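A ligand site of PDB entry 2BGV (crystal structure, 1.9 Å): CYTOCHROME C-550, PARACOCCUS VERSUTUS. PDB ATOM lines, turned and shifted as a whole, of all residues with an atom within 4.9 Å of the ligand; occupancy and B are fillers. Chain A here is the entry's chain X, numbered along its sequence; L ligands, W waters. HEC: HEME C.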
ATOM      1  N   PHE A  12      31.152  -3.319  -2.469  1.00  0.00           N
ATOM      2  CA  PHE A  12      30.226  -4.035  -3.349  1.00  0.00           C
ATOM      3  C   PHE A  12      30.383  -3.604  -4.814  1.00  0.00           C
ATOM      4  O   PHE A  12      29.952  -4.317  -5.745  1.00  0.00           O
ATOM      5  CB  PHE A  12      28.778  -3.819  -2.893  1.00  0.00           C
ATOM      6  CG  PHE A  12      27.802  -4.708  -3.618  1.00  0.00           C
ATOM      7  CD1 PHE A  12      27.644  -6.028  -3.249  1.00  0.00           C
ATOM      8  CD2 PHE A  12      27.117  -4.248  -4.735  1.00  0.00           C
ATOM      9  CE1 PHE A  12      26.742  -6.883  -3.933  1.00  0.00           C
ATOM     10  CE2 PHE A  12      26.220  -5.100  -5.454  1.00  0.00           C
ATOM     11  CZ  PHE A  12      26.046  -6.411  -5.033  1.00  0.00           C
ATOM     12  N   LYS A  14      32.882  -3.988  -6.394  1.00  0.00           N
ATOM     13  CA  LYS A  14      33.587  -5.107  -7.009  1.00  0.00           C
ATOM     14  C   LYS A  14      32.633  -6.213  -7.509  1.00  0.00           C
ATOM     15  O   LYS A  14      33.002  -7.028  -8.337  1.00  0.00           O
ATOM     16  CB  LYS A  14      34.610  -5.685  -6.044  1.00  0.00           C
ATOM     17  CG  LYS A  14      35.842  -4.793  -5.784  1.00  0.00           C
ATOM     18  CD  LYS A  14      36.576  -5.215  -4.517  1.00  0.00           C
ATOM     19  CE  LYS A  14      37.689  -4.257  -4.126  1.00  0.00           C
ATOM     20  NZ  LYS A  14      38.429  -4.776  -2.909  1.00  0.00           N
ATOM     21  N   CYS A  15      31.409  -6.239  -6.965  1.00  0.00           N
ATOM     22  CA  CYS A  15      30.431  -7.283  -7.285  1.00  0.00           C
ATOM     23  C   CYS A  15      29.454  -6.860  -8.370  1.00  0.00           C
ATOM     24  O   CYS A  15      28.759  -7.697  -8.966  1.00  0.00           O
ATOM     25  CB  CYS A  15      29.605  -7.621  -6.049  1.00  0.00           C
ATOM     26  SG  CYS A  15      30.562  -7.892  -4.536  1.00  0.00           S
ATOM     27  N   CYS A  18      28.320  -8.166 -11.992  1.00  0.00           N
ATOM     28  CA  CYS A  18      27.513  -9.371 -12.166  1.00  0.00           C
ATOM     29  C   CYS A  18      26.235  -9.439 -11.322  1.00  0.00           C
ATOM     30  O   CYS A  18      25.404 -10.318 -11.552  1.00  0.00           O
ATOM     31  CB  CYS A  18      28.353 -10.587 -11.814  1.00  0.00           C
ATOM     32  SG  CYS A  18      29.867 -10.711 -12.855  1.00  0.00           S
ATOM     33  N   HIS A  19      26.131  -8.601 -10.294  1.00  0.00           N
ATOM     34  CA  HIS A  19      25.008  -8.698  -9.351  1.00  0.00           C
ATOM     35  C   HIS A  19      24.402  -7.337  -9.116  1.00  0.00           C
ATOM     36  O   HIS A  19      25.105  -6.361  -8.997  1.00  0.00           O
ATOM     37  CB  HIS A  19      25.478  -9.165  -7.980  1.00  0.00           C
ATOM     38  CG  HIS A  19      25.973 -10.568  -7.949  1.00  0.00           C
ATOM     39  ND1 HIS A  19      25.139 -11.659  -7.913  1.00  0.00           N
ATOM     40  CD2 HIS A  19      27.245 -11.052  -7.823  1.00  0.00           C
ATOM     41  CE1 HIS A  19      25.869 -12.753  -7.751  1.00  0.00           C
ATOM     42  NE2 HIS A  19      27.150 -12.410  -7.724  1.00  0.00           N
ATOM     43  N   THR A  35      24.531 -11.320 -14.669  1.00  0.00           N
ATOM     44  CA  THR A  35      25.284 -12.562 -14.812  1.00  0.00           C
ATOM     45  C   THR A  35      25.058 -13.494 -13.621  1.00  0.00           C
ATOM     46  O   THR A  35      24.935 -14.692 -13.797  1.00  0.00           O
ATOM     47  CB  THR A  35      26.778 -12.282 -14.993  1.00  0.00           C
ATOM     48  OG1 THR A  35      26.947 -11.531 -16.206  1.00  0.00           O
ATOM     49  CG2 THR A  35      27.591 -13.566 -15.113  1.00  0.00           C
ATOM     50  N   GLY A  36      25.051 -12.939 -12.410  1.00  0.00           N
ATOM     51  CA  GLY A  36      24.729 -13.680 -11.197  1.00  0.00           C
ATOM     52  C   GLY A  36      23.370 -13.196 -10.662  1.00  0.00           C
ATOM     53  O   GLY A  36      22.839 -12.225 -11.158  1.00  0.00           O
ATOM     54  N   PRO A  37      22.787 -13.924  -9.689  1.00  0.00           N
ATOM     55  CA  PRO A  37      21.457 -13.593  -9.165  1.00  0.00           C
ATOM     56  C   PRO A  37      21.392 -12.290  -8.409  1.00  0.00           C
ATOM     57  O   PRO A  37      22.391 -11.807  -7.879  1.00  0.00           O
ATOM     58  CB  PRO A  37      21.134 -14.753  -8.208  1.00  0.00           C
ATOM     59  CG  PRO A  37      22.201 -15.753  -8.376  1.00  0.00           C
ATOM     60  CD  PRO A  37      23.354 -15.133  -9.092  1.00  0.00           C
ATOM     61  N   LEU A  39      20.923 -10.053  -5.368  1.00  0.00           N
ATOM     62  CA  LEU A  39      21.366 -10.316  -4.002  1.00  0.00           C
ATOM     63  C   LEU A  39      20.539  -9.596  -2.940  1.00  0.00           C
ATOM     64  O   LEU A  39      20.793  -9.752  -1.747  1.00  0.00           O
ATOM     65  CB  LEU A  39      22.835  -9.969  -3.835  1.00  0.00           C
ATOM     66  CG  LEU A  39      23.808 -10.810  -4.661  1.00  0.00           C
ATOM     67  CD1 LEU A  39      25.230 -10.399  -4.372  1.00  0.00           C
ATOM     68  CD2 LEU A  39      23.589 -12.289  -4.392  1.00  0.00           C
ATOM     69  N   VAL A  42      19.421 -11.827   0.182  1.00  0.00           N
ATOM     70  CA  VAL A  42      20.202 -13.063   0.138  1.00  0.00           C
ATOM     71  C   VAL A  42      20.514 -13.628   1.519  1.00  0.00           C
ATOM     72  O   VAL A  42      20.574 -14.841   1.696  1.00  0.00           O
ATOM     73  CB  VAL A  42      21.503 -12.928  -0.696  1.00  0.00           C
ATOM     74  CG1 VAL A  42      22.481 -11.970  -0.017  1.00  0.00           C
ATOM     75  CG2 VAL A  42      22.122 -14.291  -0.951  1.00  0.00           C
ATOM     76  N   ARG A  45      18.174 -16.388   2.901  1.00  0.00           N
ATOM     77  CA  ARG A  45      17.538 -17.009   1.735  1.00  0.00           C
ATOM     78  C   ARG A  45      18.003 -18.437   1.586  1.00  0.00           C
ATOM     79  O   ARG A  45      19.191 -18.725   1.799  1.00  0.00           O
ATOM     80  CB  ARG A  45      17.972 -16.274   0.461  1.00  0.00           C
ATOM     81  CG  ARG A  45      17.260 -16.631  -0.777  1.00  0.00           C
ATOM     82  CD  ARG A  45      17.293 -15.449  -1.766  1.00  0.00           C
ATOM     83  NE  ARG A  45      18.516 -15.452  -2.553  1.00  0.00           N
ATOM     84  CZ  ARG A  45      18.911 -14.443  -3.306  1.00  0.00           C
ATOM     85  NH1 ARG A  45      18.202 -13.322  -3.357  1.00  0.00           N
ATOM     86  NH2 ARG A  45      20.019 -14.554  -4.030  1.00  0.00           N
ATOM     87  N   ILE A  47      19.635 -21.551  -0.129  1.00  0.00           N
ATOM     88  CA  ILE A  47      20.777 -21.628  -1.038  1.00  0.00           C
ATOM     89  C   ILE A  47      20.250 -21.868  -2.442  1.00  0.00           C
ATOM     90  O   ILE A  47      19.369 -22.704  -2.617  1.00  0.00           O
ATOM     91  CB  ILE A  47      21.682 -22.816  -0.664  1.00  0.00           C
ATOM     92  CG1 ILE A  47      22.231 -22.664   0.740  1.00  0.00           C
ATOM     93  CG2 ILE A  47      22.795 -23.014  -1.693  1.00  0.00           C
ATOM     94  CD1 ILE A  47      22.939 -21.411   1.020  1.00  0.00           C
ATOM     95  N   ALA A  48      20.719 -21.092  -3.409  1.00  0.00           N
ATOM     96  CA  ALA A  48      20.404 -21.318  -4.823  1.00  0.00           C
ATOM     97  C   ALA A  48      18.919 -21.450  -5.123  1.00  0.00           C
ATOM     98  O   ALA A  48      18.491 -22.423  -5.763  1.00  0.00           O
ATOM     99  CB  ALA A  48      21.137 -22.522  -5.336  1.00  0.00           C
ATOM    100  N   SER A  49      18.139 -20.474  -4.697  1.00  0.00           N
ATOM    101  CA  SER A  49      16.685 -20.587  -4.759  1.00  0.00           C
ATOM    102  C   SER A  49      16.002 -19.489  -5.573  1.00  0.00           C
ATOM    103  O   SER A  49      14.771 -19.395  -5.576  1.00  0.00           O
ATOM    104  CB  SER A  49      16.130 -20.602  -3.342  1.00  0.00           C
ATOM    105  OG  SER A  49      16.313 -19.347  -2.721  1.00  0.00           O
ATOM    106  N   VAL A  50      16.773 -18.640  -6.241  1.00  0.00           N
ATOM    107  CA  VAL A  50      16.172 -17.627  -7.110  1.00  0.00           C
ATOM    108  C   VAL A  50      15.573 -18.311  -8.333  1.00  0.00           C
ATOM    109  O   VAL A  50      16.280 -18.934  -9.134  1.00  0.00           O
ATOM    110  CB  VAL A  50      17.184 -16.499  -7.520  1.00  0.00           C
ATOM    111  CG1 VAL A  50      16.527 -15.500  -8.518  1.00  0.00           C
ATOM    112  CG2 VAL A  50      17.657 -15.737  -6.308  1.00  0.00           C
ATOM    113  N   PHE A  53      16.891 -18.373 -12.282  1.00  0.00           N
ATOM    114  CA  PHE A  53      18.341 -18.344 -12.458  1.00  0.00           C
ATOM    115  C   PHE A  53      18.904 -19.732 -12.725  1.00  0.00           C
ATOM    116  O   PHE A  53      18.573 -20.700 -12.059  1.00  0.00           O
ATOM    117  CB  PHE A  53      19.036 -17.672 -11.271  1.00  0.00           C
ATOM    118  CG  PHE A  53      20.499 -17.434 -11.510  1.00  0.00           C
ATOM    119  CD1 PHE A  53      20.911 -16.355 -12.275  1.00  0.00           C
ATOM    120  CD2 PHE A  53      21.434 -18.387 -11.132  1.00  0.00           C
ATOM    121  CE1 PHE A  53      22.245 -16.176 -12.567  1.00  0.00           C
ATOM    122  CE2 PHE A  53      22.774 -18.201 -11.383  1.00  0.00           C
ATOM    123  CZ  PHE A  53      23.178 -17.097 -12.127  1.00  0.00           C
ATOM    124  N   LYS A  54      19.794 -19.826 -13.703  1.00  0.00           N
ATOM    125  CA  LYS A  54      20.406 -21.091 -14.042  1.00  0.00           C
ATOM    126  C   LYS A  54      21.697 -21.306 -13.233  1.00  0.00           C
ATOM    127  O   LYS A  54      22.787 -20.908 -13.646  1.00  0.00           O
ATOM    128  CB  LYS A  54      20.641 -21.176 -15.543  1.00  0.00           C
ATOM    129  CG  LYS A  54      19.302 -21.171 -16.336  1.00  0.00           C
ATOM    130  CD  LYS A  54      19.416 -20.548 -17.722  1.00  0.00           C
ATOM    131  CE  LYS A  54      18.022 -20.175 -18.301  1.00  0.00           C
ATOM    132  NZ  LYS A  54      17.304 -21.346 -18.883  1.00  0.00           N
ATOM    133  N   TYR A  55      21.548 -21.901 -12.066  1.00  0.00           N
ATOM    134  CA  TYR A  55      22.682 -22.123 -11.179  1.00  0.00           C
ATOM    135  C   TYR A  55      23.543 -23.258 -11.689  1.00  0.00           C
ATOM    136  O   TYR A  55      23.087 -24.109 -12.449  1.00  0.00           O
ATOM    137  CB  TYR A  55      22.209 -22.480  -9.775  1.00  0.00           C
ATOM    138  CG  TYR A  55      21.610 -21.336  -9.001  1.00  0.00           C
ATOM    139  CD1 TYR A  55      22.416 -20.450  -8.314  1.00  0.00           C
ATOM    140  CD2 TYR A  55      20.204 -21.181  -8.917  1.00  0.00           C
ATOM    141  CE1 TYR A  55      21.862 -19.411  -7.586  1.00  0.00           C
ATOM    142  CE2 TYR A  55      19.656 -20.171  -8.197  1.00  0.00           C
ATOM    143  CZ  TYR A  55      20.457 -19.271  -7.528  1.00  0.00           C
ATOM    144  OH  TYR A  55      19.886 -18.283  -6.752  1.00  0.00           O
ATOM    145  N   GLY A  56      24.800 -23.261 -11.238  1.00  0.00           N
ATOM    146  CA  GLY A  56      25.716 -24.355 -11.497  1.00  0.00           C
ATOM    147  C   GLY A  56      25.388 -25.591 -10.693  1.00  0.00           C
ATOM    148  O   GLY A  56      24.672 -25.539  -9.699  1.00  0.00           O
ATOM    149  N   ILE A  59      26.486 -25.777  -6.586  1.00  0.00           N
ATOM    150  CA  ILE A  59      25.648 -25.099  -5.592  1.00  0.00           C
ATOM    151  C   ILE A  59      24.269 -25.756  -5.495  1.00  0.00           C
ATOM    152  O   ILE A  59      23.702 -25.861  -4.403  1.00  0.00           O
ATOM    153  CB  ILE A  59      25.569 -23.578  -5.882  1.00  0.00           C
ATOM    154  CG1 ILE A  59      25.056 -22.813  -4.641  1.00  0.00           C
ATOM    155  CG2 ILE A  59      24.712 -23.276  -7.115  1.00  0.00           C
ATOM    156  CD1 ILE A  59      25.296 -21.313  -4.740  1.00  0.00           C
ATOM    157  N   TRP A  71      21.334 -19.114   3.584  1.00  0.00           N
ATOM    158  CA  TRP A  71      22.611 -18.414   3.675  1.00  0.00           C
ATOM    159  C   TRP A  71      22.734 -17.807   5.066  1.00  0.00           C
ATOM    160  O   TRP A  71      21.971 -16.893   5.423  1.00  0.00           O
ATOM    161  CB  TRP A  71      22.720 -17.307   2.625  1.00  0.00           C
ATOM    162  CG  TRP A  71      23.061 -17.796   1.280  1.00  0.00           C
ATOM    163  CD1 TRP A  71      22.266 -17.783   0.176  1.00  0.00           C
ATOM    164  CD2 TRP A  71      24.303 -18.397   0.880  1.00  0.00           C
ATOM    165  NE1 TRP A  71      22.930 -18.308  -0.891  1.00  0.00           N
ATOM    166  CE2 TRP A  71      24.192 -18.696  -0.489  1.00  0.00           C
ATOM    167  CE3 TRP A  71      25.492 -18.744   1.551  1.00  0.00           C
ATOM    168  CZ2 TRP A  71      25.209 -19.309  -1.206  1.00  0.00           C
ATOM    169  CZ3 TRP A  71      26.499 -19.351   0.842  1.00  0.00           C
ATOM    170  CH2 TRP A  71      26.367 -19.613  -0.535  1.00  0.00           C
ATOM    171  N   LEU A  76      28.141 -17.057   4.031  1.00  0.00           N
ATOM    172  CA  LEU A  76      28.374 -16.006   3.037  1.00  0.00           C
ATOM    173  C   LEU A  76      29.837 -15.491   3.072  1.00  0.00           C
ATOM    174  O   LEU A  76      30.470 -15.287   2.033  1.00  0.00           O
ATOM    175  CB  LEU A  76      27.402 -14.844   3.214  1.00  0.00           C
ATOM    176  CG  LEU A  76      26.008 -15.167   2.655  1.00  0.00           C
ATOM    177  CD1 LEU A  76      24.998 -14.169   3.197  1.00  0.00           C
ATOM    178  CD2 LEU A  76      25.992 -15.155   1.107  1.00  0.00           C
ATOM    179  N   TYR A  79      31.991 -18.208   1.487  1.00  0.00           N
ATOM    180  CA  TYR A  79      31.727 -18.308   0.055  1.00  0.00           C
ATOM    181  C   TYR A  79      32.307 -17.146  -0.747  1.00  0.00           C
ATOM    182  O   TYR A  79      32.933 -17.366  -1.805  1.00  0.00           O
ATOM    183  CB  TYR A  79      30.214 -18.435  -0.182  1.00  0.00           C
ATOM    184  CG  TYR A  79      29.797 -18.533  -1.632  1.00  0.00           C
ATOM    185  CD1 TYR A  79      29.815 -19.754  -2.297  1.00  0.00           C
ATOM    186  CD2 TYR A  79      29.350 -17.414  -2.336  1.00  0.00           C
ATOM    187  CE1 TYR A  79      29.411 -19.852  -3.623  1.00  0.00           C
ATOM    188  CE2 TYR A  79      28.937 -17.510  -3.663  1.00  0.00           C
ATOM    189  CZ  TYR A  79      28.990 -18.738  -4.301  1.00  0.00           C
ATOM    190  OH  TYR A  79      28.586 -18.873  -5.607  1.00  0.00           O
ATOM    191  N   VAL A  80      32.111 -15.922  -0.270  1.00  0.00           N
ATOM    192  CA  VAL A  80      32.619 -14.768  -1.015  1.00  0.00           C
ATOM    193  C   VAL A  80      34.165 -14.661  -0.958  1.00  0.00           C
ATOM    194  O   VAL A  80      34.774 -14.027  -1.825  1.00  0.00           O
ATOM    195  CB  VAL A  80      31.995 -13.450  -0.579  1.00  0.00           C
ATOM    196  CG1 VAL A  80      30.474 -13.474  -0.824  1.00  0.00           C
ATOM    197  CG2 VAL A  80      32.324 -13.113   0.835  1.00  0.00           C
ATOM    198  N   LYS A  97      31.242 -28.027  -9.612  1.00  0.00           N
ATOM    199  CA  LYS A  97      31.150 -26.910 -10.550  1.00  0.00           C
ATOM    200  C   LYS A  97      30.785 -25.628  -9.827  1.00  0.00           C
ATOM    201  O   LYS A  97      29.863 -25.622  -9.042  1.00  0.00           O
ATOM    202  CB  LYS A  97      30.072 -27.198 -11.588  1.00  0.00           C
ATOM    203  CG  LYS A  97      29.725 -26.008 -12.438  1.00  0.00           C
ATOM    204  CD  LYS A  97      30.874 -25.655 -13.389  1.00  0.00           C
ATOM    205  CE  LYS A  97      30.552 -24.465 -14.271  1.00  0.00           C
ATOM    206  NZ  LYS A  97      31.643 -24.191 -15.296  1.00  0.00           N
ATOM    207  N   THR A  98      31.493 -24.553 -10.153  1.00  0.00           N
ATOM    208  CA  THR A  98      31.115 -23.220  -9.749  1.00  0.00           C
ATOM    209  C   THR A  98      30.999 -22.301 -10.958  1.00  0.00           C
ATOM    210  O   THR A  98      31.851 -22.306 -11.825  1.00  0.00           O
ATOM    211  CB  THR A  98      32.082 -22.629  -8.702  1.00  0.00           C
ATOM    212  OG1 THR A  98      31.549 -21.396  -8.242  1.00  0.00           O
ATOM    213  CG2 THR A  98      33.466 -22.404  -9.264  1.00  0.00           C
ATOM    214  N   LYS A  99      29.919 -21.530 -11.045  1.00  0.00           N
ATOM    215  CA  LYS A  99      29.810 -20.496 -12.064  1.00  0.00           C
ATOM    216  C   LYS A  99      30.416 -19.176 -11.619  1.00  0.00           C
ATOM    217  O   LYS A  99      30.581 -18.271 -12.439  1.00  0.00           O
ATOM    218  CB  LYS A  99      28.357 -20.313 -12.526  1.00  0.00           C
ATOM    219  CG  LYS A  99      27.871 -21.496 -13.296  1.00  0.00           C
ATOM    220  CD  LYS A  99      26.438 -21.336 -13.790  1.00  0.00           C
ATOM    221  CE  LYS A  99      26.253 -20.153 -14.698  1.00  0.00           C
ATOM    222  NZ  LYS A  99      24.845 -20.117 -15.195  1.00  0.00           N
ATOM    223  N   MET A 100      30.785 -19.079 -10.339  1.00  0.00           N
ATOM    224  CA  MET A 100      31.374 -17.875  -9.812  1.00  0.00           C
ATOM    225  C   MET A 100      32.780 -18.195  -9.305  1.00  0.00           C
ATOM    226  O   MET A 100      32.943 -19.029  -8.431  1.00  0.00           O
ATOM    227  CB  MET A 100      30.546 -17.329  -8.660  1.00  0.00           C
ATOM    228  CG  MET A 100      31.080 -16.022  -8.099  1.00  0.00           C
ATOM    229  SD  MET A 100      30.124 -15.450  -6.672  1.00  0.00           S
ATOM    230  CE  MET A 100      31.422 -14.660  -5.749  1.00  0.00           C
ATOM    231  N   PHE A 102      35.080 -15.408  -8.845  1.00  0.00           N
ATOM    232  CA  PHE A 102      35.582 -14.181  -8.254  1.00  0.00           C
ATOM    233  C   PHE A 102      35.870 -14.366  -6.776  1.00  0.00           C
ATOM    234  O   PHE A 102      35.053 -14.941  -6.026  1.00  0.00           O
ATOM    235  CB  PHE A 102      34.564 -13.047  -8.435  1.00  0.00           C
ATOM    236  CG  PHE A 102      35.089 -11.709  -8.047  1.00  0.00           C
ATOM    237  CD1 PHE A 102      34.972 -11.260  -6.741  1.00  0.00           C
ATOM    238  CD2 PHE A 102      35.660 -10.869  -8.987  1.00  0.00           C
ATOM    239  CE1 PHE A 102      35.450 -10.012  -6.376  1.00  0.00           C
ATOM    240  CE2 PHE A 102      36.122  -9.613  -8.638  1.00  0.00           C
ATOM    241  CZ  PHE A 102      36.068  -9.201  -7.322  1.00  0.00           C
ATOM    242  N   LEU A 104      37.052 -12.581  -3.050  1.00  0.00           N
ATOM    243  CA  LEU A 104      37.207 -11.376  -2.246  1.00  0.00           C
ATOM    244  C   LEU A 104      38.008 -11.730  -0.989  1.00  0.00           C
ATOM    245  O   LEU A 104      37.492 -12.381  -0.076  1.00  0.00           O
ATOM    246  CB  LEU A 104      35.852 -10.787  -1.867  1.00  0.00           C
ATOM    247  CG  LEU A 104      35.877  -9.421  -1.140  1.00  0.00           C
ATOM    248  CD1 LEU A 104      36.376  -8.277  -2.048  1.00  0.00           C
ATOM    249  CD2 LEU A 104      34.504  -9.104  -0.553  1.00  0.00           C
ATOM    250  N   VAL A 111      31.068  -6.540   3.450  1.00  0.00           N
ATOM    251  CA  VAL A 111      30.156  -6.748   2.320  1.00  0.00           C
ATOM    252  C   VAL A 111      28.927  -7.542   2.741  1.00  0.00           C
ATOM    253  O   VAL A 111      27.797  -7.192   2.363  1.00  0.00           O
ATOM    254  CB  VAL A 111      30.858  -7.446   1.163  1.00  0.00           C
ATOM    255  CG1 VAL A 111      29.861  -7.884   0.126  1.00  0.00           C
ATOM    256  CG2 VAL A 111      31.895  -6.509   0.572  1.00  0.00           C
ATOM    257  N   LEU A 115      24.833  -6.536   2.672  1.00  0.00           N
ATOM    258  CA  LEU A 115      23.765  -7.383   2.136  1.00  0.00           C
ATOM    259  C   LEU A 115      22.689  -7.652   3.204  1.00  0.00           C
ATOM    260  O   LEU A 115      21.518  -7.734   2.889  1.00  0.00           O
ATOM    261  CB  LEU A 115      24.357  -8.689   1.592  1.00  0.00           C
ATOM    262  CG  LEU A 115      25.297  -8.471   0.388  1.00  0.00           C
ATOM    263  CD1 LEU A 115      25.933  -9.774   0.035  1.00  0.00           C
ATOM    264  CD2 LEU A 115      24.522  -7.908  -0.807  1.00  0.00           C
HETATM  265 FE   HEC L   1      28.577 -13.754  -7.263  1.00  0.00          FE
HETATM  266  CHA HEC L   1      26.544 -16.458  -7.036  1.00  0.00           C
HETATM  267  CHB HEC L   1      27.888 -12.981  -3.994  1.00  0.00           C
HETATM  268  CHC HEC L   1      30.985 -11.330  -7.366  1.00  0.00           C
HETATM  269  CHD HEC L   1      28.833 -14.157 -10.624  1.00  0.00           C
HETATM  270  NA  HEC L   1      27.433 -14.570  -5.781  1.00  0.00           N
HETATM  271  C1A HEC L   1      26.680 -15.723  -5.890  1.00  0.00           C
HETATM  272  C2A HEC L   1      25.997 -15.947  -4.618  1.00  0.00           C
HETATM  273  C3A HEC L   1      26.394 -14.978  -3.774  1.00  0.00           C
HETATM  274  C4A HEC L   1      27.300 -14.108  -4.482  1.00  0.00           C
HETATM  275  CMA HEC L   1      25.972 -14.816  -2.297  1.00  0.00           C
HETATM  276  CAA HEC L   1      24.996 -17.091  -4.301  1.00  0.00           C
HETATM  277  CBA HEC L   1      23.622 -16.564  -4.723  1.00  0.00           C
HETATM  278  CGA HEC L   1      22.450 -17.487  -4.459  1.00  0.00           C
HETATM  279  O1A HEC L   1      21.327 -17.175  -4.930  1.00  0.00           O
HETATM  280  O2A HEC L   1      22.609 -18.525  -3.784  1.00  0.00           O
HETATM  281  NB  HEC L   1      29.291 -12.428  -5.939  1.00  0.00           N
HETATM  282  C1B HEC L   1      28.827 -12.219  -4.668  1.00  0.00           C
HETATM  283  C2B HEC L   1      29.536 -11.096  -4.095  1.00  0.00           C
HETATM  284  C3B HEC L   1      30.383 -10.641  -5.019  1.00  0.00           C
HETATM  285  C4B HEC L   1      30.261 -11.475  -6.192  1.00  0.00           C
HETATM  286  CMB HEC L   1      29.251 -10.547  -2.689  1.00  0.00           C
HETATM  287  CAB HEC L   1      31.391  -9.493  -4.887  1.00  0.00           C
HETATM  288  CBB HEC L   1      32.260  -9.650  -3.864  1.00  0.00           C
HETATM  289  NC  HEC L   1      29.759 -12.942  -8.729  1.00  0.00           N
HETATM  290  C1C HEC L   1      30.656 -11.898  -8.570  1.00  0.00           C
HETATM  291  C2C HEC L   1      31.143 -11.508  -9.879  1.00  0.00           C
HETATM  292  C3C HEC L   1      30.546 -12.304 -10.796  1.00  0.00           C
HETATM  293  C4C HEC L   1      29.642 -13.203 -10.073  1.00  0.00           C
HETATM  294  CMC HEC L   1      32.152 -10.389 -10.148  1.00  0.00           C
HETATM  295  CAC HEC L   1      30.702 -12.298 -12.324  1.00  0.00           C
HETATM  296  CBC HEC L   1      31.948 -12.341 -12.831  1.00  0.00           C
HETATM  297  ND  HEC L   1      27.798 -15.061  -8.610  1.00  0.00           N
HETATM  298  C1D HEC L   1      28.089 -15.076  -9.964  1.00  0.00           C
HETATM  299  C2D HEC L   1      27.435 -16.215 -10.583  1.00  0.00           C
HETATM  300  C3D HEC L   1      26.757 -16.942  -9.457  1.00  0.00           C
HETATM  301  C4D HEC L   1      27.029 -16.168  -8.270  1.00  0.00           C
HETATM  302  CMD HEC L   1      27.484 -16.616 -12.063  1.00  0.00           C
HETATM  303  CAD HEC L   1      26.000 -18.268  -9.522  1.00  0.00           C
HETATM  304  CBD HEC L   1      26.955 -19.310  -8.918  1.00  0.00           C
HETATM  305  CGD HEC L   1      26.688 -20.717  -9.407  1.00  0.00           C
HETATM  306  O1D HEC L   1      25.561 -20.966  -9.916  1.00  0.00           O
HETATM  307  O2D HEC L   1      27.592 -21.588  -9.253  1.00  0.00           O
HETATM  308  O   HOH W   1      29.217 -21.128  -6.911  1.00  0.00           O
HETATM  309  O   HOH W   2      19.501 -18.102  -2.988  1.00  0.00           O
HETATM  310  O   HOH W   3      27.590 -24.264  -8.799  1.00  0.00           O
HETATM  311  O   HOH W   4      31.157 -15.649 -13.148  1.00  0.00           O
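The side-chain sulfur (SG) of Cys 15 is bonded to a carbon (CAB) of the ligand.
A carbon (CAC) of the ligand is covalently linked to the side-chain sulfur of Cys 18 (1.9 Å).
A ring nitrogen (NE2) of His 19 is bound to an iron atom (FE) of the ligand (2.0 Å).
SD of Met 100 binds FE of the ligand.
OH of Tyr 55 is in hydrogen-bond range of O1A of the ligand, at 2.6 Å.
An oxygen (O1D) of the ligand is in hydrogen-bond range of the backbone NH of Gly 56 (2.8 Å).
NE1 of Trp 71 is in hydrogen-bond range of O2A of the ligand (2.9 Å).
O2D of the ligand is in hydrogen-bond range of N of Lys 99.
O1A of the ligand is in salt-bridge range of NH2 of Arg 45, 3.1 Å away.
N of Ala 48 sits at hydrogen-bond distance from O2A of the ligand (3.2 Å).
Residues that only touch the ligand: Leu 76 (3.4 Å), Tyr 79 (3.5 Å), Thr 35 (3.6 Å), Val 80 (3.7 Å), Leu 39 (3.7 Å), Phe 53 (3.7 Å), Phe 102 (3.7 Å), Ile 59 (3.7 Å), Gly 36 (3.8 Å), Pro 37 (3.8 Å), Thr 98 (3.9 Å), Lys 14 (3.9 Å) and Val 111 (3.9 Å).
23 residues have an atom within 4 Å of the ligand: Lys 14, Cys 15, Cys 18, His 19, Thr 35, Gly 36, Pro 37, Leu 39, Arg 45, Ala 48, Phe 53, Tyr 55, Gly 56, Ile 59, Trp 71, Leu 76, Tyr 79, Val 80, Thr 98, Lys 99, Met 100, Phe 102 and Val 111.
O of Cys 18 sits at hydrogen-bond distance from N of Thr 35.
The backbone carbonyl oxygen of Cys 18 sits at hydrogen-bond distance from the backbone NH of Gly 36 (2.8 Å).
The side-chain hydroxyl (OG1) of Thr 98 is in hydrogen-bond range of the backbone carbonyl oxygen (O) of Met 100.
The backbone NH (N) of Val 50 lies within hydrogen-bond range of the side-chain hydroxyl (OH) of Tyr 55, 3.2 Å away.
N of Ser 49 lies within hydrogen-bond range of OH of Tyr 55 (3.5 Å).
N of Trp 71 sits at hydrogen-bond distance from O of Arg 45 (2.8 Å).
The side-chain amino group of Lys 99 lies within hydrogen-bond range of the backbone carbonyl oxygen of Lys 54, 2.7 Å away.
The backbone carbonyl oxygen (O) of Val 80 sits at hydrogen-bond distance from the backbone NH (N) of Leu 104, 3.0 Å away.
Water W3 lies within hydrogen-bond range of the backbone carbonyl oxygen of Lys 97 (2.7 Å), an oxygen (O2D) of the ligand (2.7 Å), the backbone NH of Ile 59 (2.9 Å) and the backbone carbonyl oxygen of Gly 56 (3.3 Å).
Water W1 lies within hydrogen-bond range of the side-chain hydroxyl (OH) of Tyr 79 (2.7 Å), the side-chain hydroxyl (OG1) of Thr 98 (2.7 Å) and an oxygen (O2D) of the ligand (2.9 Å).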
